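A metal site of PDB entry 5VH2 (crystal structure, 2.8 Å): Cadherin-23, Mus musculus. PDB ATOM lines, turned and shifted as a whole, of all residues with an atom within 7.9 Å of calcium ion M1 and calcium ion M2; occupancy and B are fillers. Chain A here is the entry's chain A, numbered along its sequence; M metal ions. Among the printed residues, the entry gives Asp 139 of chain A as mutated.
OE1 of Glu 20 sits close to N of Tyr 73 (2.6 Å).
The backbone carbonyl oxygen of Leu 104 sits at hydrogen-bond distance from the backbone NH of Glu 20, at 3.3 Å.
The side-chain carboxylate (OE2) of Glu 106 sits at hydrogen-bond distance from the side-chain hydroxyl (OG1) of Thr 21 (2.4 Å).
The backbone NH (N) of Glu 109 lies within hydrogen-bond range of the side-chain carboxylate (OD2) of Asp 141, 2.9 Å away.
The side-chain carboxylate (OD1) of Asp 139 is in hydrogen-bond range of the backbone NH (N) of Asp 141.
OD2 of Asp 72 sits at hydrogen-bond distance from OG1 of Thr 75, 2.7 Å away.
Of the 20 residues printed, 5 come within 4 Å of calcium ion M1.
Of the 20 residues printed, 6 come within 4 Å of calcium ion M2.
The nearest printed residue that does not touch calcium ion M2 is Glu 109 (4.2 Å).
Calcium ion M2 is bound by OD1 of Asn 105 (2.2 Å).
Calcium ion M2 is bound by OE2 of Glu 20 (2.2 Å).
Calcium ion M2 is bound by the backbone carbonyl oxygen (O) of Glu 106 (2.3 Å).
The side-chain carboxylate (OD1) of Asp 141 is bound to calcium ion M2 (2.5 Å).
The side-chain carboxylate (OD1) of Asp 108 binds calcium ion M2.
OE1 of Glu 74 is bound to calcium ion M2 (2.7 Å).
Calcium ion M2 is bound by OE2 of Glu 74, at 2.8 Å.
Calcium ion M2 has seven donor atoms within binding distance.
Calcium ion M1 is bound by OE2 of Glu 74 (2.0 Å), OE1 of Glu 109 (2.3 Å), OD1 of Asp 72 (2.5 Å), OD2 of Asp 108 (2.6 Å), OD1 of Asp 108 (2.6 Å) and OE1 of Glu 20 (2.7 Å).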
ATOM      1  N   GLU A  20     -30.851  12.688   5.190  1.00  0.00           N
ATOM      2  CA  GLU A  20     -30.160  12.998   6.461  1.00  0.00           C
ATOM      3  C   GLU A  20     -28.972  13.934   6.268  1.00  0.00           C
ATOM      4  O   GLU A  20     -28.654  14.702   7.181  1.00  0.00           O
ATOM      5  CB  GLU A  20     -29.729  11.727   7.225  1.00  0.00           C
ATOM      6  CG  GLU A  20     -28.655  10.935   6.542  1.00  0.00           C
ATOM      7  CD  GLU A  20     -27.967   9.909   7.426  1.00  0.00           C
ATOM      8  OE1 GLU A  20     -27.664  10.184   8.621  1.00  0.00           O
ATOM      9  OE2 GLU A  20     -27.678   8.807   6.892  1.00  0.00           O
ATOM     10  N   THR A  21     -28.357  13.896   5.085  1.00  0.00           N
ATOM     11  CA  THR A  21     -27.246  14.811   4.755  1.00  0.00           C
ATOM     12  C   THR A  21     -27.713  16.144   4.189  1.00  0.00           C
ATOM     13  O   THR A  21     -26.900  16.914   3.672  1.00  0.00           O
ATOM     14  CB  THR A  21     -26.231  14.186   3.752  1.00  0.00           C
ATOM     15  OG1 THR A  21     -26.867  13.948   2.486  1.00  0.00           O
ATOM     16  CG2 THR A  21     -25.628  12.899   4.296  1.00  0.00           C
ATOM     17  N   LEU A  71     -28.428  16.846  10.435  1.00  0.00           N
ATOM     18  CA  LEU A  71     -29.244  15.709  10.810  1.00  0.00           C
ATOM     19  C   LEU A  71     -28.404  14.458  10.765  1.00  0.00           C
ATOM     20  O   LEU A  71     -27.279  14.489  10.253  1.00  0.00           O
ATOM     21  CB  LEU A  71     -30.468  15.577   9.896  1.00  0.00           C
ATOM     22  CG  LEU A  71     -31.372  16.803   9.849  1.00  0.00           C
ATOM     23  CD1 LEU A  71     -32.268  16.724   8.627  1.00  0.00           C
ATOM     24  CD2 LEU A  71     -32.192  16.871  11.129  1.00  0.00           C
ATOM     25  N   ASP A  72     -28.915  13.412  11.433  1.00  0.00           N
ATOM     26  CA  ASP A  72     -28.242  12.134  11.459  1.00  0.00           C
ATOM     27  C   ASP A  72     -29.236  10.980  11.644  1.00  0.00           C
ATOM     28  O   ASP A  72     -29.857  10.818  12.723  1.00  0.00           O
ATOM     29  CB  ASP A  72     -27.189  12.169  12.559  1.00  0.00           C
ATOM     30  CG  ASP A  72     -26.264  10.967  12.543  1.00  0.00           C
ATOM     31  OD1 ASP A  72     -26.280  10.179  11.548  1.00  0.00           O
ATOM     32  OD2 ASP A  72     -25.503  10.852  13.536  1.00  0.00           O
ATOM     33  N   TYR A  73     -29.384  10.161  10.596  1.00  0.00           N
ATOM     34  CA  TYR A  73     -30.187   8.953  10.653  1.00  0.00           C
ATOM     35  C   TYR A  73     -29.754   8.049  11.805  1.00  0.00           C
ATOM     36  O   TYR A  73     -30.581   7.523  12.563  1.00  0.00           O
ATOM     37  CB  TYR A  73     -30.080   8.187   9.358  1.00  0.00           C
ATOM     38  CG  TYR A  73     -30.982   6.993   9.273  1.00  0.00           C
ATOM     39  CD1 TYR A  73     -32.308   7.129   8.851  1.00  0.00           C
ATOM     40  CD2 TYR A  73     -30.540   5.728   9.581  1.00  0.00           C
ATOM     41  CE1 TYR A  73     -33.159   6.049   8.761  1.00  0.00           C
ATOM     42  CE2 TYR A  73     -31.398   4.619   9.497  1.00  0.00           C
ATOM     43  CZ  TYR A  73     -32.708   4.796   9.088  1.00  0.00           C
ATOM     44  OH  TYR A  73     -33.589   3.741   8.988  1.00  0.00           O
ATOM     45  N   GLU A  74     -28.449   7.911  11.947  1.00  0.00           N
ATOM     46  CA  GLU A  74     -27.847   7.040  12.955  1.00  0.00           C
ATOM     47  C   GLU A  74     -27.964   7.562  14.378  1.00  0.00           C
ATOM     48  O   GLU A  74     -27.704   6.810  15.298  1.00  0.00           O
ATOM     49  CB  GLU A  74     -26.379   6.781  12.622  1.00  0.00           C
ATOM     50  CG  GLU A  74     -26.109   5.767  11.494  1.00  0.00           C
ATOM     51  CD  GLU A  74     -26.435   6.274  10.085  1.00  0.00           C
ATOM     52  OE1 GLU A  74     -26.829   5.435   9.247  1.00  0.00           O
ATOM     53  OE2 GLU A  74     -26.301   7.484   9.797  1.00  0.00           O
ATOM     54  N   THR A  75     -28.328   8.826  14.594  1.00  0.00           N
ATOM     55  CA  THR A  75     -28.644   9.341  15.949  1.00  0.00           C
ATOM     56  C   THR A  75     -30.149   9.476  16.200  1.00  0.00           C
ATOM     57  O   THR A  75     -30.592   9.269  17.323  1.00  0.00           O
ATOM     58  CB  THR A  75     -28.013  10.709  16.192  1.00  0.00           C
ATOM     59  OG1 THR A  75     -26.598  10.625  16.022  1.00  0.00           O
ATOM     60  CG2 THR A  75     -28.350  11.226  17.627  1.00  0.00           C
ATOM     61  N   LEU A 104     -34.118   9.842   5.590  1.00  0.00           N
ATOM     62  CA  LEU A 104     -33.658   8.859   4.627  1.00  0.00           C
ATOM     63  C   LEU A 104     -32.209   8.539   4.972  1.00  0.00           C
ATOM     64  O   LEU A 104     -31.357   9.416   4.951  1.00  0.00           O
ATOM     65  CB  LEU A 104     -33.796   9.422   3.212  1.00  0.00           C
ATOM     66  CG  LEU A 104     -33.050   8.765   2.040  1.00  0.00           C
ATOM     67  CD1 LEU A 104     -33.486   7.334   1.880  1.00  0.00           C
ATOM     68  CD2 LEU A 104     -33.348   9.536   0.771  1.00  0.00           C
ATOM     69  N   ASN A 105     -31.936   7.300   5.355  1.00  0.00           N
ATOM     70  CA  ASN A 105     -30.556   6.849   5.549  1.00  0.00           C
ATOM     71  C   ASN A 105     -29.782   6.976   4.239  1.00  0.00           C
ATOM     72  O   ASN A 105     -30.208   6.504   3.205  1.00  0.00           O
ATOM     73  CB  ASN A 105     -30.543   5.413   6.034  1.00  0.00           C
ATOM     74  CG  ASN A 105     -29.142   4.960   6.437  1.00  0.00           C
ATOM     75  OD1 ASN A 105     -28.237   5.762   6.717  1.00  0.00           O
ATOM     76  ND2 ASN A 105     -28.961   3.637   6.465  1.00  0.00           N
ATOM     77  N   GLU A 106     -28.672   7.692   4.303  1.00  0.00           N
ATOM     78  CA  GLU A 106     -27.762   7.783   3.182  1.00  0.00           C
ATOM     79  C   GLU A 106     -26.403   7.308   3.627  1.00  0.00           C
ATOM     80  O   GLU A 106     -26.134   7.212   4.826  1.00  0.00           O
ATOM     81  CB  GLU A 106     -27.627   9.225   2.747  1.00  0.00           C
ATOM     82  CG  GLU A 106     -28.918   9.950   2.414  1.00  0.00           C
ATOM     83  CD  GLU A 106     -28.631  11.266   1.715  1.00  0.00           C
ATOM     84  OE1 GLU A 106     -28.313  11.231   0.495  1.00  0.00           O
ATOM     85  OE2 GLU A 106     -28.663  12.322   2.384  1.00  0.00           O
ATOM     86  N   LEU A 107     -25.547   7.013   2.659  1.00  0.00           N
ATOM     87  CA  LEU A 107     -24.216   6.508   2.931  1.00  0.00           C
ATOM     88  C   LEU A 107     -23.286   7.648   3.344  1.00  0.00           C
ATOM     89  O   LEU A 107     -22.602   8.245   2.506  1.00  0.00           O
ATOM     90  CB  LEU A 107     -23.699   5.808   1.691  1.00  0.00           C
ATOM     91  CG  LEU A 107     -22.497   4.877   1.890  1.00  0.00           C
ATOM     92  CD1 LEU A 107     -22.844   3.550   2.564  1.00  0.00           C
ATOM     93  CD2 LEU A 107     -21.898   4.623   0.513  1.00  0.00           C
ATOM     94  N   ASP A 108     -23.236   7.902   4.641  1.00  0.00           N
ATOM     95  CA  ASP A 108     -22.426   8.973   5.232  1.00  0.00           C
ATOM     96  C   ASP A 108     -21.601   8.535   6.460  1.00  0.00           C
ATOM     97  O   ASP A 108     -21.157   9.368   7.232  1.00  0.00           O
ATOM     98  CB  ASP A 108     -23.350  10.131   5.632  1.00  0.00           C
ATOM     99  CG  ASP A 108     -24.311   9.772   6.767  1.00  0.00           C
ATOM    100  OD1 ASP A 108     -24.617   8.576   6.972  1.00  0.00           O
ATOM    101  OD2 ASP A 108     -24.788  10.680   7.457  1.00  0.00           O
ATOM    102  N   GLU A 109     -21.416   7.233   6.643  1.00  0.00           N
ATOM    103  CA  GLU A 109     -20.751   6.735   7.847  1.00  0.00           C
ATOM    104  C   GLU A 109     -19.664   5.734   7.487  1.00  0.00           C
ATOM    105  O   GLU A 109     -19.635   5.246   6.371  1.00  0.00           O
ATOM    106  CB  GLU A 109     -21.736   6.073   8.820  1.00  0.00           C
ATOM    107  CG  GLU A 109     -22.877   6.945   9.303  1.00  0.00           C
ATOM    108  CD  GLU A 109     -22.417   8.049  10.228  1.00  0.00           C
ATOM    109  OE1 GLU A 109     -23.270   8.875  10.584  1.00  0.00           O
ATOM    110  OE2 GLU A 109     -21.230   8.082  10.586  1.00  0.00           O
ATOM    111  N   ALA A 110     -18.825   5.409   8.475  1.00  0.00           N
ATOM    112  CA  ALA A 110     -17.665   4.561   8.276  1.00  0.00           C
ATOM    113  C   ALA A 110     -18.047   3.082   8.347  1.00  0.00           C
ATOM    114  O   ALA A 110     -19.152   2.705   7.903  1.00  0.00           O
ATOM    115  CB  ALA A 110     -16.575   4.917   9.295  1.00  0.00           C
ATOM    116  N   ASP A 139     -20.666  -2.374   7.187  1.00  0.00           N
ATOM    117  CA  ASP A 139     -21.029  -0.994   6.917  1.00  0.00           C
ATOM    118  C   ASP A 139     -21.954  -0.474   8.024  1.00  0.00           C
ATOM    119  O   ASP A 139     -23.087  -0.955   8.195  1.00  0.00           O
ATOM    120  CB  ASP A 139     -21.755  -0.922   5.571  1.00  0.00           C
ATOM    121  CG  ASP A 139     -22.267   0.441   5.239  1.00  0.00           C
ATOM    122  OD1 ASP A 139     -21.661   1.423   5.720  1.00  0.00           O
ATOM    123  OD2 ASP A 139     -23.258   0.516   4.482  1.00  0.00           O
ATOM    124  N   ILE A 140     -21.462   0.520   8.768  1.00  0.00           N
ATOM    125  CA  ILE A 140     -22.275   1.199   9.766  1.00  0.00           C
ATOM    126  C   ILE A 140     -23.614   1.633   9.197  1.00  0.00           C
ATOM    127  O   ILE A 140     -24.630   1.455   9.836  1.00  0.00           O
ATOM    128  CB  ILE A 140     -21.525   2.407  10.383  1.00  0.00           C
ATOM    129  CG1 ILE A 140     -20.378   1.911  11.275  1.00  0.00           C
ATOM    130  CG2 ILE A 140     -22.483   3.290  11.179  1.00  0.00           C
ATOM    131  CD1 ILE A 140     -19.364   2.978  11.642  1.00  0.00           C
ATOM    132  N   ASP A 141     -23.610   2.183   7.981  1.00  0.00           N
ATOM    133  CA  ASP A 141     -24.835   2.664   7.326  1.00  0.00           C
ATOM    134  C   ASP A 141     -25.872   1.596   7.026  1.00  0.00           C
ATOM    135  O   ASP A 141     -27.051   1.920   6.819  1.00  0.00           O
ATOM    136  CB  ASP A 141     -24.514   3.375   6.005  1.00  0.00           C
ATOM    137  CG  ASP A 141     -23.784   4.674   6.185  1.00  0.00           C
ATOM    138  OD1 ASP A 141     -24.412   5.701   6.562  1.00  0.00           O
ATOM    139  OD2 ASP A 141     -22.552   4.671   5.935  1.00  0.00           O
ATOM    140  N   ASN A 142     -25.423   0.324   6.967  1.00  0.00           N
ATOM    141  CA  ASN A 142     -26.289  -0.820   6.660  1.00  0.00           C
ATOM    142  C   ASN A 142     -26.920  -0.717   5.274  1.00  0.00           C
ATOM    143  O   ASN A 142     -28.033  -1.181   5.050  1.00  0.00           O
ATOM    144  CB  ASN A 142     -27.329  -0.997   7.768  1.00  0.00           C
ATOM    145  CG  ASN A 142     -26.697  -1.390   9.083  1.00  0.00           C
ATOM    146  OD1 ASN A 142     -25.644  -2.020   9.090  1.00  0.00           O
ATOM    147  ND2 ASN A 142     -27.328  -1.037  10.196  1.00  0.00           N
ATOM    148  N   LEU A 143     -26.178  -0.124   4.333  1.00  0.00           N
ATOM    149  CA  LEU A 143     -26.591  -0.024   2.938  1.00  0.00           C
ATOM    150  C   LEU A 143     -25.744  -0.915   2.025  1.00  0.00           C
ATOM    151  O   LEU A 143     -26.291  -1.663   1.234  1.00  0.00           O
ATOM    152  CB  LEU A 143     -26.487   1.409   2.477  1.00  0.00           C
ATOM    153  CG  LEU A 143     -27.350   2.466   3.213  1.00  0.00           C
ATOM    154  CD1 LEU A 143     -26.861   3.842   2.883  1.00  0.00           C
ATOM    155  CD2 LEU A 143     -28.809   2.366   2.816  1.00  0.00           C
ATOM    156  N   LYS A 197     -16.028   8.363   3.793  1.00  0.00           N
ATOM    157  CA  LYS A 197     -15.189   8.536   4.991  1.00  0.00           C
ATOM    158  C   LYS A 197     -13.692   8.311   4.802  1.00  0.00           C
ATOM    159  O   LYS A 197     -13.290   7.596   3.895  1.00  0.00           O
ATOM    160  CB  LYS A 197     -15.705   7.683   6.161  1.00  0.00           C
ATOM    161  CG  LYS A 197     -17.042   8.209   6.715  1.00  0.00           C
ATOM    162  CD  LYS A 197     -16.968   9.572   7.418  1.00  0.00           C
ATOM    163  CE  LYS A 197     -17.970   9.608   8.583  1.00  0.00           C
ATOM    164  NZ  LYS A 197     -18.292  10.988   9.048  1.00  0.00           N
HETATM  165 CA    CA M   1     -25.294   9.151   9.465  1.00  0.00          CA
HETATM  166 CA    CA M   2     -26.461   6.936   7.092  1.00  0.00          CA
